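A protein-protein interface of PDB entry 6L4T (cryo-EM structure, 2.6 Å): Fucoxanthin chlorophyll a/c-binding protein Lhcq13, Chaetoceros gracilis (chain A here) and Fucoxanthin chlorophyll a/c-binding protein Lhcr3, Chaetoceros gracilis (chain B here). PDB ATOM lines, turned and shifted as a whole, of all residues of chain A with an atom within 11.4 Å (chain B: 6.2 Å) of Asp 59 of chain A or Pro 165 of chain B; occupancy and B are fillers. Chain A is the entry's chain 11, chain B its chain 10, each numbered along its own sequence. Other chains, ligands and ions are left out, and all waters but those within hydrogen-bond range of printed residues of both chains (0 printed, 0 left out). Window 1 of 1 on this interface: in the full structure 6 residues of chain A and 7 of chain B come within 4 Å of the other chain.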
ATOM      1  N   SER A  34     -11.455  24.220   4.887  1.00  0.00           N
ATOM      2  CA  SER A  34     -12.591  25.120   5.050  1.00  0.00           C
ATOM      3  C   SER A  34     -12.684  26.097   3.885  1.00  0.00           C
ATOM      4  O   SER A  34     -13.650  26.847   3.771  1.00  0.00           O
ATOM      5  CB  SER A  34     -12.488  25.882   6.371  1.00  0.00           C
ATOM      6  OG  SER A  34     -11.500  26.894   6.300  1.00  0.00           O
ATOM      7  N   ILE A  35     -11.667  26.084   3.021  1.00  0.00           N
ATOM      8  CA  ILE A  35     -11.713  26.918   1.826  1.00  0.00           C
ATOM      9  C   ILE A  35     -12.626  26.290   0.778  1.00  0.00           C
ATOM     10  O   ILE A  35     -13.265  27.000  -0.009  1.00  0.00           O
ATOM     11  CB  ILE A  35     -10.281  27.169   1.307  1.00  0.00           C
ATOM     12  CG1 ILE A  35     -10.268  28.133   0.116  1.00  0.00           C
ATOM     13  CG2 ILE A  35      -9.565  25.863   0.973  1.00  0.00           C
ATOM     14  CD1 ILE A  35     -10.926  29.461   0.400  1.00  0.00           C
ATOM     15  N   ASN A  36     -12.761  24.963   0.784  1.00  0.00           N
ATOM     16  CA  ASN A  36     -13.651  24.300  -0.158  1.00  0.00           C
ATOM     17  C   ASN A  36     -15.107  24.330   0.288  1.00  0.00           C
ATOM     18  O   ASN A  36     -15.970  23.823  -0.434  1.00  0.00           O
ATOM     19  CB  ASN A  36     -13.201  22.855  -0.381  1.00  0.00           C
ATOM     20  CG  ASN A  36     -13.553  22.345  -1.765  1.00  0.00           C
ATOM     21  OD1 ASN A  36     -13.858  23.127  -2.666  1.00  0.00           O
ATOM     22  ND2 ASN A  36     -13.518  21.030  -1.940  1.00  0.00           N
ATOM     23  N   GLU A  37     -15.400  24.904   1.454  1.00  0.00           N
ATOM     24  CA  GLU A  37     -16.770  25.149   1.883  1.00  0.00           C
ATOM     25  C   GLU A  37     -17.043  26.634   2.088  1.00  0.00           C
ATOM     26  O   GLU A  37     -17.886  26.998   2.912  1.00  0.00           O
ATOM     27  CB  GLU A  37     -17.081  24.366   3.159  1.00  0.00           C
ATOM     28  CG  GLU A  37     -17.134  22.865   2.952  1.00  0.00           C
ATOM     29  CD  GLU A  37     -18.206  22.453   1.963  1.00  0.00           C
ATOM     30  OE1 GLU A  37     -19.397  22.712   2.234  1.00  0.00           O
ATOM     31  OE2 GLU A  37     -17.857  21.873   0.913  1.00  0.00           O
ATOM     32  N   CYS A  49     -13.493  24.076  -5.264  1.00  0.00           N
ATOM     33  CA  CYS A  49     -12.491  25.115  -5.415  1.00  0.00           C
ATOM     34  C   CYS A  49     -11.345  24.576  -6.267  1.00  0.00           C
ATOM     35  O   CYS A  49     -10.992  23.399  -6.141  1.00  0.00           O
ATOM     36  CB  CYS A  49     -11.983  25.569  -4.047  1.00  0.00           C
ATOM     37  SG  CYS A  49     -10.721  26.861  -4.071  1.00  0.00           S
ATOM     38  N   PRO A  51      -7.747  23.546  -7.637  1.00  0.00           N
ATOM     39  CA  PRO A  51      -6.747  22.978  -6.717  1.00  0.00           C
ATOM     40  C   PRO A  51      -5.536  23.859  -6.482  1.00  0.00           C
ATOM     41  O   PRO A  51      -4.955  23.800  -5.392  1.00  0.00           O
ATOM     42  CB  PRO A  51      -6.356  21.662  -7.404  1.00  0.00           C
ATOM     43  CG  PRO A  51      -6.634  21.903  -8.847  1.00  0.00           C
ATOM     44  CD  PRO A  51      -7.858  22.762  -8.879  1.00  0.00           C
ATOM     45  N   LEU A  52      -5.137  24.675  -7.456  1.00  0.00           N
ATOM     46  CA  LEU A  52      -3.989  25.544  -7.237  1.00  0.00           C
ATOM     47  C   LEU A  52      -4.356  26.703  -6.320  1.00  0.00           C
ATOM     48  O   LEU A  52      -3.491  27.234  -5.614  1.00  0.00           O
ATOM     49  CB  LEU A  52      -3.452  26.040  -8.581  1.00  0.00           C
ATOM     50  CG  LEU A  52      -2.025  26.585  -8.689  1.00  0.00           C
ATOM     51  CD1 LEU A  52      -1.494  26.287 -10.081  1.00  0.00           C
ATOM     52  CD2 LEU A  52      -1.922  28.077  -8.411  1.00  0.00           C
ATOM     53  N   GLY A  53      -5.632  27.091  -6.300  1.00  0.00           N
ATOM     54  CA  GLY A  53      -6.072  28.130  -5.388  1.00  0.00           C
ATOM     55  C   GLY A  53      -6.422  27.622  -4.008  1.00  0.00           C
ATOM     56  O   GLY A  53      -6.269  28.351  -3.024  1.00  0.00           O
ATOM     57  N   ALA A  54      -6.896  26.378  -3.906  1.00  0.00           N
ATOM     58  CA  ALA A  54      -7.183  25.807  -2.595  1.00  0.00           C
ATOM     59  C   ALA A  54      -5.909  25.402  -1.866  1.00  0.00           C
ATOM     60  O   ALA A  54      -5.928  25.219  -0.645  1.00  0.00           O
ATOM     61  CB  ALA A  54      -8.114  24.603  -2.734  1.00  0.00           C
ATOM     62  N   ARG A  55      -4.795  25.270  -2.590  1.00  0.00           N
ATOM     63  CA  ARG A  55      -3.530  24.889  -1.969  1.00  0.00           C
ATOM     64  C   ARG A  55      -2.924  26.034  -1.168  1.00  0.00           C
ATOM     65  O   ARG A  55      -2.002  25.813  -0.377  1.00  0.00           O
ATOM     66  CB  ARG A  55      -2.545  24.419  -3.037  1.00  0.00           C
ATOM     67  CG  ARG A  55      -2.451  22.915  -3.186  1.00  0.00           C
ATOM     68  CD  ARG A  55      -1.140  22.519  -3.847  1.00  0.00           C
ATOM     69  NE  ARG A  55      -0.977  21.069  -3.919  1.00  0.00           N
ATOM     70  CZ  ARG A  55      -1.303  20.334  -4.976  1.00  0.00           C
ATOM     71  NH1 ARG A  55      -1.811  20.910  -6.056  1.00  0.00           N
ATOM     72  NH2 ARG A  55      -1.120  19.022  -4.953  1.00  0.00           N
ATOM     73  N   ILE A  56      -3.414  27.258  -1.365  1.00  0.00           N
ATOM     74  CA  ILE A  56      -2.888  28.399  -0.632  1.00  0.00           C
ATOM     75  C   ILE A  56      -3.643  28.634   0.669  1.00  0.00           C
ATOM     76  O   ILE A  56      -3.053  29.104   1.649  1.00  0.00           O
ATOM     77  CB  ILE A  56      -2.931  29.653  -1.525  1.00  0.00           C
ATOM     78  CG1 ILE A  56      -2.559  29.290  -2.961  1.00  0.00           C
ATOM     79  CG2 ILE A  56      -1.988  30.724  -1.005  1.00  0.00           C
ATOM     80  CD1 ILE A  56      -2.629  30.452  -3.922  1.00  0.00           C
ATOM     81  N   LEU A  57      -4.934  28.299   0.720  1.00  0.00           N
ATOM     82  CA  LEU A  57      -5.791  28.736   1.815  1.00  0.00           C
ATOM     83  C   LEU A  57      -6.362  27.586   2.639  1.00  0.00           C
ATOM     84  O   LEU A  57      -7.225  27.821   3.490  1.00  0.00           O
ATOM     85  CB  LEU A  57      -6.932  29.597   1.274  1.00  0.00           C
ATOM     86  CG  LEU A  57      -6.549  30.909   0.593  1.00  0.00           C
ATOM     87  CD1 LEU A  57      -7.789  31.621   0.094  1.00  0.00           C
ATOM     88  CD2 LEU A  57      -5.776  31.790   1.553  1.00  0.00           C
ATOM     89  N   GLU A  58      -5.914  26.349   2.422  1.00  0.00           N
ATOM     90  CA  GLU A  58      -6.515  25.242   3.162  1.00  0.00           C
ATOM     91  C   GLU A  58      -5.899  25.117   4.553  1.00  0.00           C
ATOM     92  O   GLU A  58      -6.576  24.720   5.510  1.00  0.00           O
ATOM     93  CB  GLU A  58      -6.411  23.935   2.355  1.00  0.00           C
ATOM     94  CG  GLU A  58      -5.259  22.981   2.666  1.00  0.00           C
ATOM     95  CD  GLU A  58      -3.990  23.307   1.900  1.00  0.00           C
ATOM     96  OE1 GLU A  58      -3.871  24.433   1.381  1.00  0.00           O
ATOM     97  OE2 GLU A  58      -3.105  22.430   1.820  1.00  0.00           O
ATOM     98  N   ASP A  59      -4.618  25.455   4.692  1.00  0.00           N
ATOM     99  CA  ASP A  59      -3.966  25.486   5.999  1.00  0.00           C
ATOM    100  C   ASP A  59      -3.781  26.933   6.451  1.00  0.00           C
ATOM    101  O   ASP A  59      -2.669  27.431   6.616  1.00  0.00           O
ATOM    102  CB  ASP A  59      -2.640  24.735   5.946  1.00  0.00           C
ATOM    103  CG  ASP A  59      -2.824  23.237   5.788  1.00  0.00           C
ATOM    104  OD1 ASP A  59      -3.858  22.715   6.252  1.00  0.00           O
ATOM    105  OD2 ASP A  59      -1.936  22.584   5.203  1.00  0.00           O
ATOM    106  N   ALA A  60      -4.906  27.611   6.660  1.00  0.00           N
ATOM    107  CA  ALA A  60      -4.868  29.026   6.996  1.00  0.00           C
ATOM    108  C   ALA A  60      -6.061  29.380   7.870  1.00  0.00           C
ATOM    109  O   ALA A  60      -7.005  28.601   8.020  1.00  0.00           O
ATOM    110  CB  ALA A  60      -4.837  29.897   5.738  1.00  0.00           C
ATOM    111  N   GLN A  61      -6.003  30.580   8.439  1.00  0.00           N
ATOM    112  CA  GLN A  61      -7.026  31.053   9.351  1.00  0.00           C
ATOM    113  C   GLN A  61      -8.288  31.443   8.584  1.00  0.00           C
ATOM    114  O   GLN A  61      -8.247  31.637   7.368  1.00  0.00           O
ATOM    115  CB  GLN A  61      -6.494  32.244  10.143  1.00  0.00           C
ATOM    116  CG  GLN A  61      -5.400  31.894  11.116  1.00  0.00           C
ATOM    117  CD  GLN A  61      -4.615  33.107  11.542  1.00  0.00           C
ATOM    118  OE1 GLN A  61      -5.170  34.190  11.710  1.00  0.00           O
ATOM    119  NE2 GLN A  61      -3.312  32.937  11.708  1.00  0.00           N
ATOM    120  N   PRO A  62      -9.434  31.546   9.270  1.00  0.00           N
ATOM    121  CA  PRO A  62     -10.629  32.098   8.612  1.00  0.00           C
ATOM    122  C   PRO A  62     -10.496  33.555   8.214  1.00  0.00           C
ATOM    123  O   PRO A  62     -11.246  34.011   7.344  1.00  0.00           O
ATOM    124  CB  PRO A  62     -11.726  31.911   9.667  1.00  0.00           C
ATOM    125  CG  PRO A  62     -11.274  30.754  10.458  1.00  0.00           C
ATOM    126  CD  PRO A  62      -9.785  30.874  10.537  1.00  0.00           C
ATOM    127  N   SER A  63      -9.580  34.306   8.827  1.00  0.00           N
ATOM    128  CA  SER A  63      -9.307  35.663   8.378  1.00  0.00           C
ATOM    129  C   SER A  63      -8.565  35.689   7.051  1.00  0.00           C
ATOM    130  O   SER A  63      -8.624  36.697   6.342  1.00  0.00           O
ATOM    131  CB  SER A  63      -8.509  36.415   9.439  1.00  0.00           C
ATOM    132  OG  SER A  63      -7.132  36.109   9.347  1.00  0.00           O
ATOM    133  N   ALA A  64      -7.866  34.608   6.704  1.00  0.00           N
ATOM    134  CA  ALA A  64      -7.216  34.531   5.402  1.00  0.00           C
ATOM    135  C   ALA A  64      -8.234  34.355   4.290  1.00  0.00           C
ATOM    136  O   ALA A  64      -8.044  34.864   3.182  1.00  0.00           O
ATOM    137  CB  ALA A  64      -6.214  33.382   5.382  1.00  0.00           C
ATOM    138  N   ILE A  65      -9.314  33.623   4.562  1.00  0.00           N
ATOM    139  CA  ILE A  65     -10.368  33.455   3.571  1.00  0.00           C
ATOM    140  C   ILE A  65     -11.146  34.750   3.407  1.00  0.00           C
ATOM    141  O   ILE A  65     -11.483  35.146   2.286  1.00  0.00           O
ATOM    142  CB  ILE A  65     -11.285  32.288   3.973  1.00  0.00           C
ATOM    143  CG1 ILE A  65     -10.452  31.044   4.263  1.00  0.00           C
ATOM    144  CG2 ILE A  65     -12.288  31.995   2.886  1.00  0.00           C
ATOM    145  CD1 ILE A  65     -11.214  29.970   4.988  1.00  0.00           C
ATOM    146  N   PHE A  68      -9.087  37.205   1.212  1.00  0.00           N
ATOM    147  CA  PHE A  68      -9.022  36.938  -0.218  1.00  0.00           C
ATOM    148  C   PHE A  68     -10.391  37.042  -0.871  1.00  0.00           C
ATOM    149  O   PHE A  68     -10.481  37.393  -2.051  1.00  0.00           O
ATOM    150  CB  PHE A  68      -8.410  35.561  -0.464  1.00  0.00           C
ATOM    151  CG  PHE A  68      -6.912  35.567  -0.495  1.00  0.00           C
ATOM    152  CD1 PHE A  68      -6.231  35.599  -1.697  1.00  0.00           C
ATOM    153  CD2 PHE A  68      -6.184  35.559   0.681  1.00  0.00           C
ATOM    154  CE1 PHE A  68      -4.852  35.611  -1.724  1.00  0.00           C
ATOM    155  CE2 PHE A  68      -4.808  35.572   0.662  1.00  0.00           C
ATOM    156  CZ  PHE A  68      -4.141  35.598  -0.541  1.00  0.00           C
ATOM    157  N   ASP B 159       0.443  39.677  10.932  1.00  0.00           N
ATOM    158  CA  ASP B 159      -0.120  38.744   9.958  1.00  0.00           C
ATOM    159  C   ASP B 159      -1.460  39.281   9.490  1.00  0.00           C
ATOM    160  O   ASP B 159      -2.519  38.842   9.951  1.00  0.00           O
ATOM    161  CB  ASP B 159      -0.271  37.349  10.556  1.00  0.00           C
ATOM    162  CG  ASP B 159      -0.532  36.302   9.511  1.00  0.00           C
ATOM    163  OD1 ASP B 159      -0.141  36.513   8.347  1.00  0.00           O
ATOM    164  OD2 ASP B 159      -1.139  35.270   9.851  1.00  0.00           O
ATOM    165  N   GLY B 162      -3.511  36.556   7.308  1.00  0.00           N
ATOM    166  CA  GLY B 162      -3.955  35.343   7.970  1.00  0.00           C
ATOM    167  C   GLY B 162      -3.270  34.065   7.542  1.00  0.00           C
ATOM    168  O   GLY B 162      -3.831  32.986   7.729  1.00  0.00           O
ATOM    169  N   LEU B 163      -2.064  34.151   6.986  1.00  0.00           N
ATOM    170  CA  LEU B 163      -1.419  32.987   6.393  1.00  0.00           C
ATOM    171  C   LEU B 163      -0.787  32.053   7.414  1.00  0.00           C
ATOM    172  O   LEU B 163      -0.381  30.949   7.041  1.00  0.00           O
ATOM    173  CB  LEU B 163      -0.361  33.436   5.393  1.00  0.00           C
ATOM    174  CG  LEU B 163      -0.902  34.114   4.143  1.00  0.00           C
ATOM    175  CD1 LEU B 163       0.233  34.746   3.374  1.00  0.00           C
ATOM    176  CD2 LEU B 163      -1.640  33.112   3.283  1.00  0.00           C
ATOM    177  N   TYR B 164      -0.685  32.464   8.666  1.00  0.00           N
ATOM    178  CA  TYR B 164      -0.148  31.604   9.711  1.00  0.00           C
ATOM    179  C   TYR B 164      -1.162  30.514  10.021  1.00  0.00           C
ATOM    180  O   TYR B 164      -2.304  30.834  10.371  1.00  0.00           O
ATOM    181  CB  TYR B 164       0.157  32.438  10.945  1.00  0.00           C
ATOM    182  CG  TYR B 164       1.155  31.839  11.901  1.00  0.00           C
ATOM    183  CD1 TYR B 164       2.323  31.252  11.441  1.00  0.00           C
ATOM    184  CD2 TYR B 164       0.953  31.914  13.270  1.00  0.00           C
ATOM    185  CE1 TYR B 164       3.246  30.729  12.314  1.00  0.00           C
ATOM    186  CE2 TYR B 164       1.870  31.393  14.151  1.00  0.00           C
ATOM    187  CZ  TYR B 164       3.015  30.802  13.668  1.00  0.00           C
ATOM    188  OH  TYR B 164       3.930  30.280  14.548  1.00  0.00           O
ATOM    189  N   PRO B 165      -0.812  29.237   9.880  1.00  0.00           N
ATOM    190  CA  PRO B 165      -1.802  28.166  10.053  1.00  0.00           C
ATOM    191  C   PRO B 165      -2.226  28.016  11.506  1.00  0.00           C
ATOM    192  O   PRO B 165      -1.658  28.605  12.423  1.00  0.00           O
ATOM    193  CB  PRO B 165      -1.076  26.919   9.548  1.00  0.00           C
ATOM    194  CG  PRO B 165       0.360  27.256   9.602  1.00  0.00           C
ATOM    195  CD  PRO B 165       0.471  28.724   9.374  1.00  0.00           C
ATOM    196  N   THR B 166      -3.275  27.224  11.703  1.00  0.00           N
ATOM    197  CA  THR B 166      -3.885  27.116  13.021  1.00  0.00           C
ATOM    198  C   THR B 166      -3.250  26.028  13.875  1.00  0.00           C
ATOM    199  O   THR B 166      -3.019  26.240  15.069  1.00  0.00           O
ATOM    200  CB  THR B 166      -5.386  26.857  12.885  1.00  0.00           C
ATOM    201  OG1 THR B 166      -5.598  25.699  12.069  1.00  0.00           O
ATOM    202  CG2 THR B 166      -6.068  28.052  12.241  1.00  0.00           C
ATOM    203  N   ASP B 167      -2.968  24.870  13.294  1.00  0.00           N
ATOM    204  CA  ASP B 167      -2.401  23.781  14.075  1.00  0.00           C
ATOM    205  C   ASP B 167      -0.910  24.019  14.306  1.00  0.00           C
ATOM    206  O   ASP B 167      -0.203  24.449  13.394  1.00  0.00           O
ATOM    207  CB  ASP B 167      -2.607  22.450  13.369  1.00  0.00           C
ATOM    208  CG  ASP B 167      -2.213  22.501  11.916  1.00  0.00           C
ATOM    209  OD1 ASP B 167      -2.520  23.515  11.255  1.00  0.00           O
ATOM    210  OD2 ASP B 167      -1.600  21.528  11.435  1.00  0.00           O
ATOM    211  N   PRO B 168      -0.411  23.748  15.517  1.00  0.00           N
ATOM    212  CA  PRO B 168       1.001  24.031  15.806  1.00  0.00           C
ATOM    213  C   PRO B 168       1.976  23.070  15.157  1.00  0.00           C
ATOM    214  O   PRO B 168       3.170  23.388  15.102  1.00  0.00           O
ATOM    215  CB  PRO B 168       1.071  23.928  17.334  1.00  0.00           C
ATOM    216  CG  PRO B 168      -0.033  23.014  17.690  1.00  0.00           C
ATOM    217  CD  PRO B 168      -1.134  23.277  16.709  1.00  0.00           C
ATOM    218  N   LYS B 170       2.227  22.357  12.038  1.00  0.00           N
ATOM    219  CA  LYS B 170       2.722  22.981  10.824  1.00  0.00           C
ATOM    220  C   LYS B 170       2.880  24.485  10.964  1.00  0.00           C
ATOM    221  O   LYS B 170       3.240  25.150   9.987  1.00  0.00           O
ATOM    222  CB  LYS B 170       1.814  22.655   9.633  1.00  0.00           C
ATOM    223  CG  LYS B 170       0.479  23.347   9.635  1.00  0.00           C
ATOM    224  CD  LYS B 170      -0.236  23.103   8.319  1.00  0.00           C
ATOM    225  CE  LYS B 170      -0.480  21.620   8.088  1.00  0.00           C
ATOM    226  NZ  LYS B 170      -1.500  21.080   9.025  1.00  0.00           N
ATOM    227  N   GLN B 171       2.620  25.041  12.148  1.00  0.00           N
ATOM    228  CA  GLN B 171       3.111  26.379  12.446  1.00  0.00           C
ATOM    229  C   GLN B 171       4.624  26.396  12.551  1.00  0.00           C
ATOM    230  O   GLN B 171       5.256  27.392  12.189  1.00  0.00           O
ATOM    231  CB  GLN B 171       2.507  26.896  13.747  1.00  0.00           C
ATOM    232  CG  GLN B 171       1.140  27.488  13.604  1.00  0.00           C
ATOM    233  CD  GLN B 171       0.612  28.033  14.909  1.00  0.00           C
ATOM    234  OE1 GLN B 171       1.246  27.895  15.951  1.00  0.00           O
ATOM    235  NE2 GLN B 171      -0.556  28.659  14.859  1.00  0.00           N
ATOM    236  N   MET B 174       6.150  26.328   9.153  1.00  0.00           N
ATOM    237  CA  MET B 174       6.042  27.674   8.603  1.00  0.00           C
ATOM    238  C   MET B 174       7.111  28.587   9.195  1.00  0.00           C
ATOM    239  O   MET B 174       7.677  29.428   8.489  1.00  0.00           O
ATOM    240  CB  MET B 174       4.645  28.234   8.859  1.00  0.00           C
ATOM    241  CG  MET B 174       4.392  29.588   8.238  1.00  0.00           C
ATOM    242  SD  MET B 174       4.535  29.581   6.448  1.00  0.00           S
ATOM    243  CE  MET B 174       2.829  29.314   5.989  1.00  0.00           C
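O of Gly 162 of chain B sits at hydrogen-bond distance from N of Gln 61 of chain A, at 3.3 Å.
The side-chain amide nitrogen (NE2) of Gln 61 of chain A lies within hydrogen-bond range of the backbone carbonyl oxygen (O) of Tyr 164 of chain B (2.7 Å).
The side-chain carboxylate (OD1) of Asp 59 of chain A lies within salt-bridge range of the side-chain amino group (NZ) of Lys 170 of chain B (3.99 Å).
The backbone NH (N) of Leu 163 of chain B lies within hydrogen-bond range of the side-chain carboxylate (OD2) of Asp 159 of chain B.
The side-chain carboxylate of Asp 159 of chain B is in hydrogen-bond range of the backbone NH of Tyr 164 of chain B (3.1 Å).
The backbone carbonyl oxygen (O) of Pro 165 of chain B sits at hydrogen-bond distance from the side-chain amide nitrogen (NE2) of Gln 171 of chain B, 2.7 Å away.
The side-chain amino group (NZ) of Lys 170 of chain B lies within salt-bridge range of the side-chain carboxylate (OD2) of Asp 167 of chain B, at 2.5 Å.
Asp 59 of chain A touches Pro 165 of chain B.
CB of Ala 60 of chain A touches O of Gly 162 of chain B, at 3.8 Å.
Gln 61 of chain A touches Asp 159 of chain B (NE2 to OD2, 3.7 Å).
CA of Gly 162 of chain B touches OG of Ser 63 of chain A, at 3.5 Å.
Ala 64 of chain A touches Gly 162 of chain B (CB to O, 3.4 Å).
Of chain B, only Pro 165 and Lys 170 come within 4 Å of Asp 59 of chain A.
Of chain A, only Asp 59 comes within 4 Å of Pro 165 of chain B.
Tyr 164 of chain B touches just one residue of chain A: Gln 61.
No residue of chain A comes within 4 Å of Thr 166 of chain B.
No residue of chain A comes within 4 Å of Asp 167 of chain B.
Lys 170 of chain B touches one residue of chain A.
No residue of chain A comes within 4 Å of Gln 171 of chain B.
Of the printed residues of chain B, Gln 61 of chain A touches Asp 159, Gly 162 and Tyr 164.
Printed residues of chain A within 4 Å of Asp 159 of chain B: Gln 61 (3.7 Å).
Of the printed residues of chain B, Ala 64 of chain A touches Gly 162.
Phe 68 of chain A touches none of the printed residues of chain B.
The nearest residue of chain A that does not touch Pro 165 of chain B is Ala 60 of chain A (4.4 Å).
Hydrophobic or aromatic side chains of chain B within 4 Å of the printed part of chain A: Tyr 164 and Pro 165.
Among the printed residues, 8 pairs touch across the chains.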
